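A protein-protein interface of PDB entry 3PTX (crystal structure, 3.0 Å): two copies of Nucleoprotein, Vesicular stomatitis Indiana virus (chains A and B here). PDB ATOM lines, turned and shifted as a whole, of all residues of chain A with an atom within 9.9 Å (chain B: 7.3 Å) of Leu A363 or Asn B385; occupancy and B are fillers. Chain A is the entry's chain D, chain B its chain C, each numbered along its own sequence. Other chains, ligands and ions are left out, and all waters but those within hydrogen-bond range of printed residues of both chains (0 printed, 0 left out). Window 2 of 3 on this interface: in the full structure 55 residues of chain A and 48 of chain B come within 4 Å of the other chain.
O of Ala A341 is in hydrogen-bond range of NH2 of Arg B386, at 3.0 Å.
Among the printed residues, merely in contact across the chains: Ser A339 with Arg B386, Ser A339 with Lys B387, Leu A343 with Arg B386, Lys A353 with Gly B379, Lys A353 with Glu B382, Leu A363 with Asn B385 and Pro A368 with Lys B387.
The backbone NH of Arg B386 is in hydrogen-bond range of the backbone carbonyl oxygen of Phe B381 (3.2 Å). The side-chain carboxylate (OE1) of Glu B382 is in salt-bridge range of the guanidinium group (NE) of Arg B386 (3.8 Å). O of Tyr A335 lies within hydrogen-bond range of OG of Ser A339, at 2.7 Å. The backbone carbonyl oxygen (O) of Ala A336 lies within hydrogen-bond range of the side-chain hydroxyl (OG) of Ser A339 (3.3 Å).
1 position is printed for both chains. Of the 8 pairs that touch across the chains among the printed residues, none has its exchanged pair printed and touching as well.
Of the 10 printed residues of chain B, 5 touch a printed residue of chain A. Hydrophobic or aromatic side chains of chain A within 4 Å of the printed part of chain B: Leu A363 and Pro A368. Along chain A the printed residues that touch a printed residue of chain B span positions 339 to 368. Among the printed residues, 8 pairs touch across the chains. Among the printed residues, no Asp or Glu carboxylate lies within 4 Å of a Lys or Arg side-chain nitrogen of the other chain.
Printed residues of chain B within 4 Å of Leu A343: Arg B386. Printed residues of chain B within 4 Å of Lys A353: Gly B379 and Glu B382. Of the printed residues of chain B, Leu A363 touches Asn B385. Thr A364 touches none of the printed residues of chain B. Of the printed residues of chain B, Pro A368 touches Lys B387 (3.9 Å). Trp A380 touches none of the printed residues of chain B. Of the printed residues of chain A, Gly B379 touches Lys A353. Asn B385 touches just one residue of chain A: Leu A363 (3.7 Å). Printed residues of chain A within 4 Å of Arg B386: Ser A339 (3.9 Å), Ala A341 (3.0 Å) and Leu A343 (3.9 Å).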
ATOM      1  N   TYR A 335     -24.018  -7.540   0.060  1.00  0.00           N
ATOM      2  CA  TYR A 335     -23.142  -6.422   0.370  1.00  0.00           C
ATOM      3  C   TYR A 335     -23.094  -6.174   1.879  1.00  0.00           C
ATOM      4  O   TYR A 335     -22.030  -6.276   2.491  1.00  0.00           O
ATOM      5  CB  TYR A 335     -23.561  -5.166  -0.375  1.00  0.00           C
ATOM      6  CG  TYR A 335     -22.526  -4.079  -0.282  1.00  0.00           C
ATOM      7  CD1 TYR A 335     -22.890  -2.756  -0.143  1.00  0.00           C
ATOM      8  CD2 TYR A 335     -21.180  -4.382  -0.308  1.00  0.00           C
ATOM      9  CE1 TYR A 335     -21.937  -1.756  -0.053  1.00  0.00           C
ATOM     10  CE2 TYR A 335     -20.222  -3.389  -0.213  1.00  0.00           C
ATOM     11  CZ  TYR A 335     -20.606  -2.084  -0.091  1.00  0.00           C
ATOM     12  OH  TYR A 335     -19.653  -1.102  -0.001  1.00  0.00           O
ATOM     13  N   ALA A 336     -24.239  -5.883   2.489  1.00  0.00           N
ATOM     14  CA  ALA A 336     -24.291  -5.723   3.948  1.00  0.00           C
ATOM     15  C   ALA A 336     -23.381  -6.753   4.591  1.00  0.00           C
ATOM     16  O   ALA A 336     -22.267  -6.440   5.001  1.00  0.00           O
ATOM     17  CB  ALA A 336     -25.735  -5.850   4.485  1.00  0.00           C
ATOM     18  N   GLY A 338     -21.392  -8.725   3.576  1.00  0.00           N
ATOM     19  CA  GLY A 338     -20.109  -8.999   2.976  1.00  0.00           C
ATOM     20  C   GLY A 338     -19.119  -8.019   3.486  1.00  0.00           C
ATOM     21  O   GLY A 338     -18.243  -8.361   4.273  1.00  0.00           O
ATOM     22  N   SER A 339     -19.290  -6.793   3.011  1.00  0.00           N
ATOM     23  CA  SER A 339     -18.453  -5.653   3.334  1.00  0.00           C
ATOM     24  C   SER A 339     -18.223  -5.535   4.841  1.00  0.00           C
ATOM     25  O   SER A 339     -17.084  -5.584   5.308  1.00  0.00           O
ATOM     26  CB  SER A 339     -19.131  -4.391   2.813  1.00  0.00           C
ATOM     27  OG  SER A 339     -20.412  -4.260   3.416  1.00  0.00           O
ATOM     28  N   SER A 340     -19.300  -5.376   5.602  1.00  0.00           N
ATOM     29  CA  SER A 340     -19.161  -5.229   7.043  1.00  0.00           C
ATOM     30  C   SER A 340     -19.120  -6.590   7.745  1.00  0.00           C
ATOM     31  O   SER A 340     -20.158  -7.145   8.116  1.00  0.00           O
ATOM     32  CB  SER A 340     -20.281  -4.346   7.603  1.00  0.00           C
ATOM     33  OG  SER A 340     -21.532  -4.998   7.529  1.00  0.00           O
ATOM     34  N   ALA A 341     -17.914  -7.120   7.924  1.00  0.00           N
ATOM     35  CA  ALA A 341     -17.740  -8.462   8.467  1.00  0.00           C
ATOM     36  C   ALA A 341     -18.265  -8.552   9.895  1.00  0.00           C
ATOM     37  O   ALA A 341     -19.164  -7.806  10.284  1.00  0.00           O
ATOM     38  CB  ALA A 341     -16.274  -8.870   8.411  1.00  0.00           C
ATOM     39  N   LEU A 343     -16.248  -9.193  12.881  1.00  0.00           N
ATOM     40  CA  LEU A 343     -15.121  -9.296  13.801  1.00  0.00           C
ATOM     41  C   LEU A 343     -15.543  -8.958  15.228  1.00  0.00           C
ATOM     42  O   LEU A 343     -16.456  -8.161  15.443  1.00  0.00           O
ATOM     43  CB  LEU A 343     -13.982  -8.375  13.357  1.00  0.00           C
ATOM     44  CG  LEU A 343     -13.153  -8.850  12.162  1.00  0.00           C
ATOM     45  CD1 LEU A 343     -12.102  -9.857  12.604  1.00  0.00           C
ATOM     46  CD2 LEU A 343     -14.051  -9.442  11.087  1.00  0.00           C
ATOM     47  N   LYS A 353     -11.032  -5.534  23.323  1.00  0.00           N
ATOM     48  CA  LYS A 353     -11.362  -4.304  22.597  1.00  0.00           C
ATOM     49  C   LYS A 353     -12.717  -3.698  22.964  1.00  0.00           C
ATOM     50  O   LYS A 353     -13.725  -3.939  22.303  1.00  0.00           O
ATOM     51  CB  LYS A 353     -11.218  -4.430  21.074  1.00  0.00           C
ATOM     52  CG  LYS A 353     -10.946  -3.076  20.424  1.00  0.00           C
ATOM     53  CD  LYS A 353     -11.382  -2.997  18.988  1.00  0.00           C
ATOM     54  CE  LYS A 353     -12.638  -2.145  18.796  1.00  0.00           C
ATOM     55  NZ  LYS A 353     -12.357  -0.680  18.775  1.00  0.00           N
ATOM     56  N   ASP A 357     -15.070   3.709  21.164  1.00  0.00           N
ATOM     57  CA  ASP A 357     -14.040   4.740  21.306  1.00  0.00           C
ATOM     58  C   ASP A 357     -14.605   6.115  21.653  1.00  0.00           C
ATOM     59  O   ASP A 357     -13.939   6.921  22.301  1.00  0.00           O
ATOM     60  CB  ASP A 357     -13.242   4.827  20.007  1.00  0.00           C
ATOM     61  CG  ASP A 357     -14.100   4.552  18.779  1.00  0.00           C
ATOM     62  OD1 ASP A 357     -14.181   3.371  18.359  1.00  0.00           O
ATOM     63  OD2 ASP A 357     -14.698   5.513  18.243  1.00  0.00           O
ATOM     64  N   LEU A 363     -18.119   8.032  11.260  1.00  0.00           N
ATOM     65  CA  LEU A 363     -17.980   8.653   9.948  1.00  0.00           C
ATOM     66  C   LEU A 363     -19.238   9.442   9.634  1.00  0.00           C
ATOM     67  O   LEU A 363     -20.346   9.033  10.003  1.00  0.00           O
ATOM     68  CB  LEU A 363     -17.727   7.601   8.856  1.00  0.00           C
ATOM     69  CG  LEU A 363     -17.045   8.062   7.555  1.00  0.00           C
ATOM     70  CD1 LEU A 363     -16.317   6.895   6.909  1.00  0.00           C
ATOM     71  CD2 LEU A 363     -17.992   8.743   6.544  1.00  0.00           C
ATOM     72  N   THR A 364     -19.063  10.573   8.953  1.00  0.00           N
ATOM     73  CA  THR A 364     -20.199  11.418   8.594  1.00  0.00           C
ATOM     74  C   THR A 364     -20.969  10.891   7.365  1.00  0.00           C
ATOM     75  O   THR A 364     -22.070  10.352   7.522  1.00  0.00           O
ATOM     76  CB  THR A 364     -19.833  12.963   8.515  1.00  0.00           C
ATOM     77  OG1 THR A 364     -21.003  13.764   8.747  1.00  0.00           O
ATOM     78  CG2 THR A 364     -19.188  13.348   7.179  1.00  0.00           C
ATOM     79  N   THR A 365     -20.406  10.981   6.159  1.00  0.00           N
ATOM     80  CA  THR A 365     -21.316  10.973   5.016  1.00  0.00           C
ATOM     81  C   THR A 365     -21.326   9.761   4.075  1.00  0.00           C
ATOM     82  O   THR A 365     -20.307   9.388   3.488  1.00  0.00           O
ATOM     83  CB  THR A 365     -21.277  12.320   4.223  1.00  0.00           C
ATOM     84  OG1 THR A 365     -22.020  12.183   3.004  1.00  0.00           O
ATOM     85  CG2 THR A 365     -19.847  12.741   3.910  1.00  0.00           C
ATOM     86  N   ASN A 366     -22.512   9.163   3.966  1.00  0.00           N
ATOM     87  CA  ASN A 366     -22.835   8.144   2.960  1.00  0.00           C
ATOM     88  C   ASN A 366     -22.026   6.840   2.998  1.00  0.00           C
ATOM     89  O   ASN A 366     -22.282   5.929   2.210  1.00  0.00           O
ATOM     90  CB  ASN A 366     -22.838   8.750   1.545  1.00  0.00           C
ATOM     91  CG  ASN A 366     -24.194   8.626   0.855  1.00  0.00           C
ATOM     92  OD1 ASN A 366     -25.195   8.264   1.489  1.00  0.00           O
ATOM     93  ND2 ASN A 366     -24.234   8.933  -0.449  1.00  0.00           N
ATOM     94  N   ALA A 367     -21.057   6.749   3.904  1.00  0.00           N
ATOM     95  CA  ALA A 367     -20.338   5.500   4.092  1.00  0.00           C
ATOM     96  C   ALA A 367     -21.348   4.469   4.559  1.00  0.00           C
ATOM     97  O   ALA A 367     -22.154   4.752   5.443  1.00  0.00           O
ATOM     98  CB  ALA A 367     -19.230   5.665   5.108  1.00  0.00           C
ATOM     99  N   PRO A 368     -21.320   3.270   3.950  1.00  0.00           N
ATOM    100  CA  PRO A 368     -22.248   2.171   4.247  1.00  0.00           C
ATOM    101  C   PRO A 368     -22.348   1.868   5.742  1.00  0.00           C
ATOM    102  O   PRO A 368     -21.387   2.097   6.487  1.00  0.00           O
ATOM    103  CB  PRO A 368     -21.643   0.986   3.495  1.00  0.00           C
ATOM    104  CG  PRO A 368     -20.256   1.399   3.136  1.00  0.00           C
ATOM    105  CD  PRO A 368     -20.318   2.874   2.952  1.00  0.00           C
ATOM    106  N   PRO A 369     -23.510   1.350   6.175  1.00  0.00           N
ATOM    107  CA  PRO A 369     -23.882   1.170   7.585  1.00  0.00           C
ATOM    108  C   PRO A 369     -22.988   0.228   8.370  1.00  0.00           C
ATOM    109  O   PRO A 369     -22.418  -0.720   7.849  1.00  0.00           O
ATOM    110  CB  PRO A 369     -25.303   0.612   7.514  1.00  0.00           C
ATOM    111  CG  PRO A 369     -25.812   1.035   6.173  1.00  0.00           C
ATOM    112  CD  PRO A 369     -24.617   1.006   5.268  1.00  0.00           C
ATOM    113  N   GLN A 370     -22.910   0.499   9.662  1.00  0.00           N
ATOM    114  CA  GLN A 370     -21.981  -0.154  10.572  1.00  0.00           C
ATOM    115  C   GLN A 370     -22.157  -1.674  10.574  1.00  0.00           C
ATOM    116  O   GLN A 370     -21.202  -2.427  10.360  1.00  0.00           O
ATOM    117  CB  GLN A 370     -22.188   0.409  11.986  1.00  0.00           C
ATOM    118  CG  GLN A 370     -22.308   1.947  12.043  1.00  0.00           C
ATOM    119  CD  GLN A 370     -23.161   2.453  13.211  1.00  0.00           C
ATOM    120  OE1 GLN A 370     -24.259   1.944  13.464  1.00  0.00           O
ATOM    121  NE2 GLN A 370     -22.656   3.465  13.922  1.00  0.00           N
ATOM    122  N   GLY A 371     -23.382  -2.121  10.815  1.00  0.00           N
ATOM    123  CA  GLY A 371     -23.634  -3.534  11.010  1.00  0.00           C
ATOM    124  C   GLY A 371     -24.477  -4.158   9.932  1.00  0.00           C
ATOM    125  O   GLY A 371     -24.225  -3.927   8.757  1.00  0.00           O
ATOM    126  N   TRP A 377     -29.704  -0.519   6.648  1.00  0.00           N
ATOM    127  CA  TRP A 377     -29.308  -0.663   5.254  1.00  0.00           C
ATOM    128  C   TRP A 377     -30.367  -0.164   4.291  1.00  0.00           C
ATOM    129  O   TRP A 377     -30.060   0.573   3.368  1.00  0.00           O
ATOM    130  CB  TRP A 377     -28.905  -2.091   4.951  1.00  0.00           C
ATOM    131  CG  TRP A 377     -27.526  -2.370   5.398  1.00  0.00           C
ATOM    132  CD1 TRP A 377     -27.141  -2.816   6.619  1.00  0.00           C
ATOM    133  CD2 TRP A 377     -26.332  -2.207   4.630  1.00  0.00           C
ATOM    134  NE1 TRP A 377     -25.780  -2.957   6.661  1.00  0.00           N
ATOM    135  CE2 TRP A 377     -25.256  -2.586   5.453  1.00  0.00           C
ATOM    136  CE3 TRP A 377     -26.070  -1.785   3.317  1.00  0.00           C
ATOM    137  CZ2 TRP A 377     -23.925  -2.544   5.015  1.00  0.00           C
ATOM    138  CZ3 TRP A 377     -24.750  -1.740   2.874  1.00  0.00           C
ATOM    139  CH2 TRP A 377     -23.694  -2.118   3.725  1.00  0.00           C
ATOM    140  N   TRP A 380     -30.007   3.440   4.307  1.00  0.00           N
ATOM    141  CA  TRP A 380     -28.823   3.713   3.494  1.00  0.00           C
ATOM    142  C   TRP A 380     -29.086   3.562   2.007  1.00  0.00           C
ATOM    143  O   TRP A 380     -28.565   4.326   1.204  1.00  0.00           O
ATOM    144  CB  TRP A 380     -27.661   2.801   3.882  1.00  0.00           C
ATOM    145  CG  TRP A 380     -26.460   2.996   3.003  1.00  0.00           C
ATOM    146  CD1 TRP A 380     -25.524   3.971   3.113  1.00  0.00           C
ATOM    147  CD2 TRP A 380     -26.069   2.200   1.875  1.00  0.00           C
ATOM    148  NE1 TRP A 380     -24.571   3.839   2.133  1.00  0.00           N
ATOM    149  CE2 TRP A 380     -24.884   2.757   1.361  1.00  0.00           C
ATOM    150  CE3 TRP A 380     -26.602   1.061   1.256  1.00  0.00           C
ATOM    151  CZ2 TRP A 380     -24.226   2.219   0.255  1.00  0.00           C
ATOM    152  CZ3 TRP A 380     -25.942   0.527   0.170  1.00  0.00           C
ATOM    153  CH2 TRP A 380     -24.771   1.109  -0.322  1.00  0.00           C
ATOM    154  N   GLY B 379      -8.702  -2.491  17.292  1.00  0.00           N
ATOM    155  CA  GLY B 379      -8.778  -1.049  17.325  1.00  0.00           C
ATOM    156  C   GLY B 379      -8.411  -0.501  15.960  1.00  0.00           C
ATOM    157  O   GLY B 379      -9.223   0.139  15.304  1.00  0.00           O
ATOM    158  N   TRP B 380      -7.191  -0.776  15.517  1.00  0.00           N
ATOM    159  CA  TRP B 380      -6.739  -0.333  14.205  1.00  0.00           C
ATOM    160  C   TRP B 380      -7.739  -0.647  13.093  1.00  0.00           C
ATOM    161  O   TRP B 380      -7.952   0.141  12.170  1.00  0.00           O
ATOM    162  CB  TRP B 380      -5.396  -0.970  13.855  1.00  0.00           C
ATOM    163  CG  TRP B 380      -4.912  -0.585  12.482  1.00  0.00           C
ATOM    164  CD1 TRP B 380      -4.278   0.573  12.129  1.00  0.00           C
ATOM    165  CD2 TRP B 380      -5.036  -1.349  11.283  1.00  0.00           C
ATOM    166  NE1 TRP B 380      -3.996   0.570  10.786  1.00  0.00           N
ATOM    167  CE2 TRP B 380      -4.451  -0.599  10.248  1.00  0.00           C
ATOM    168  CE3 TRP B 380      -5.585  -2.596  10.983  1.00  0.00           C
ATOM    169  CZ2 TRP B 380      -4.404  -1.059   8.939  1.00  0.00           C
ATOM    170  CZ3 TRP B 380      -5.527  -3.054   9.686  1.00  0.00           C
ATOM    171  CH2 TRP B 380      -4.945  -2.286   8.678  1.00  0.00           C
ATOM    172  N   PHE B 381      -8.341  -1.820  13.166  1.00  0.00           N
ATOM    173  CA  PHE B 381      -9.268  -2.215  12.126  1.00  0.00           C
ATOM    174  C   PHE B 381     -10.535  -1.351  12.198  1.00  0.00           C
ATOM    175  O   PHE B 381     -10.951  -0.772  11.193  1.00  0.00           O
ATOM    176  CB  PHE B 381      -9.563  -3.723  12.202  1.00  0.00           C
ATOM    177  CG  PHE B 381     -10.209  -4.283  10.955  1.00  0.00           C
ATOM    178  CD1 PHE B 381      -9.524  -4.288   9.744  1.00  0.00           C
ATOM    179  CD2 PHE B 381     -11.499  -4.791  10.993  1.00  0.00           C
ATOM    180  CE1 PHE B 381     -10.117  -4.772   8.595  1.00  0.00           C
ATOM    181  CE2 PHE B 381     -12.098  -5.281   9.854  1.00  0.00           C
ATOM    182  CZ  PHE B 381     -11.407  -5.271   8.651  1.00  0.00           C
ATOM    183  N   GLU B 382     -11.133  -1.255  13.387  1.00  0.00           N
ATOM    184  CA  GLU B 382     -12.287  -0.387  13.585  1.00  0.00           C
ATOM    185  C   GLU B 382     -11.924   0.990  13.084  1.00  0.00           C
ATOM    186  O   GLU B 382     -12.764   1.694  12.535  1.00  0.00           O
ATOM    187  CB  GLU B 382     -12.700  -0.335  15.059  1.00  0.00           C
ATOM    188  CG  GLU B 382     -13.828  -1.302  15.442  1.00  0.00           C
ATOM    189  CD  GLU B 382     -15.214  -0.653  15.381  1.00  0.00           C
ATOM    190  OE1 GLU B 382     -16.224  -1.395  15.295  1.00  0.00           O
ATOM    191  OE2 GLU B 382     -15.289   0.599  15.423  1.00  0.00           O
ATOM    192  N   ASP B 383     -10.655   1.353  13.264  1.00  0.00           N
ATOM    193  CA  ASP B 383     -10.135   2.657  12.841  1.00  0.00           C
ATOM    194  C   ASP B 383     -10.132   2.688  11.324  1.00  0.00           C
ATOM    195  O   ASP B 383     -10.035   3.747  10.707  1.00  0.00           O
ATOM    196  CB  ASP B 383      -8.700   2.898  13.371  1.00  0.00           C
ATOM    197  CG  ASP B 383      -8.608   4.046  14.401  1.00  0.00           C
ATOM    198  OD1 ASP B 383      -8.760   5.233  14.016  1.00  0.00           O
ATOM    199  OD2 ASP B 383      -8.349   3.756  15.594  1.00  0.00           O
ATOM    200  N   GLN B 384     -10.233   1.514  10.722  1.00  0.00           N
ATOM    201  CA  GLN B 384     -10.192   1.427   9.278  1.00  0.00           C
ATOM    202  C   GLN B 384     -11.578   1.292   8.665  1.00  0.00           C
ATOM    203  O   GLN B 384     -11.730   0.825   7.539  1.00  0.00           O
ATOM    204  CB  GLN B 384      -9.304   0.276   8.848  1.00  0.00           C
ATOM    205  CG  GLN B 384      -8.193   0.736   7.940  1.00  0.00           C
ATOM    206  CD  GLN B 384      -7.176   1.579   8.663  1.00  0.00           C
ATOM    207  OE1 GLN B 384      -7.042   1.483   9.878  1.00  0.00           O
ATOM    208  NE2 GLN B 384      -6.444   2.404   7.920  1.00  0.00           N
ATOM    209  N   ASN B 385     -12.584   1.733   9.411  1.00  0.00           N
ATOM    210  CA  ASN B 385     -13.978   1.642   8.980  1.00  0.00           C
ATOM    211  C   ASN B 385     -14.403   0.179   8.779  1.00  0.00           C
ATOM    212  O   ASN B 385     -15.412  -0.110   8.128  1.00  0.00           O
ATOM    213  CB  ASN B 385     -14.248   2.533   7.750  1.00  0.00           C
ATOM    214  CG  ASN B 385     -13.905   4.013   8.004  1.00  0.00           C
ATOM    215  OD1 ASN B 385     -13.359   4.696   7.133  1.00  0.00           O
ATOM    216  ND2 ASN B 385     -14.212   4.502   9.207  1.00  0.00           N
ATOM    217  N   ARG B 386     -13.612  -0.725   9.363  1.00  0.00           N
ATOM    218  CA  ARG B 386     -13.945  -2.142   9.462  1.00  0.00           C
ATOM    219  C   ARG B 386     -13.944  -2.830   8.100  1.00  0.00           C
ATOM    220  O   ARG B 386     -14.751  -3.719   7.842  1.00  0.00           O
ATOM    221  CB  ARG B 386     -15.296  -2.316  10.156  1.00  0.00           C
ATOM    222  CG  ARG B 386     -15.322  -1.858  11.621  1.00  0.00           C
ATOM    223  CD  ARG B 386     -15.192  -3.031  12.600  1.00  0.00           C
ATOM    224  NE  ARG B 386     -16.338  -3.941  12.517  1.00  0.00           N
ATOM    225  CZ  ARG B 386     -16.440  -4.969  11.669  1.00  0.00           C
ATOM    226  NH1 ARG B 386     -15.461  -5.245  10.818  1.00  0.00           N
ATOM    227  NH2 ARG B 386     -17.528  -5.726  11.673  1.00  0.00           N
ATOM    228  N   LYS B 387     -13.014  -2.415   7.246  1.00  0.00           N
ATOM    229  CA  LYS B 387     -12.939  -2.864   5.859  1.00  0.00           C
ATOM    230  C   LYS B 387     -11.469  -2.944   5.473  1.00  0.00           C
ATOM    231  O   LYS B 387     -10.782  -1.925   5.454  1.00  0.00           O
ATOM    232  CB  LYS B 387     -13.646  -1.860   4.942  1.00  0.00           C
ATOM    233  CG  LYS B 387     -14.364  -2.460   3.747  1.00  0.00           C
ATOM    234  CD  LYS B 387     -15.733  -1.807   3.559  1.00  0.00           C
ATOM    235  CE  LYS B 387     -16.567  -1.913   4.845  1.00  0.00           C
ATOM    236  NZ  LYS B 387     -17.969  -1.420   4.689  1.00  0.00           N
ATOM    237  N   PRO B 388     -10.990  -4.146   5.125  1.00  0.00           N
ATOM    238  CA  PRO B 388      -9.558  -4.415   4.933  1.00  0.00           C
ATOM    239  C   PRO B 388      -8.851  -3.479   3.939  1.00  0.00           C
ATOM    240  O   PRO B 388      -9.343  -3.205   2.846  1.00  0.00           O
ATOM    241  CB  PRO B 388      -9.537  -5.866   4.442  1.00  0.00           C
ATOM    242  CG  PRO B 388     -10.863  -6.090   3.864  1.00  0.00           C
ATOM    243  CD  PRO B 388     -11.821  -5.268   4.664  1.00  0.00           C
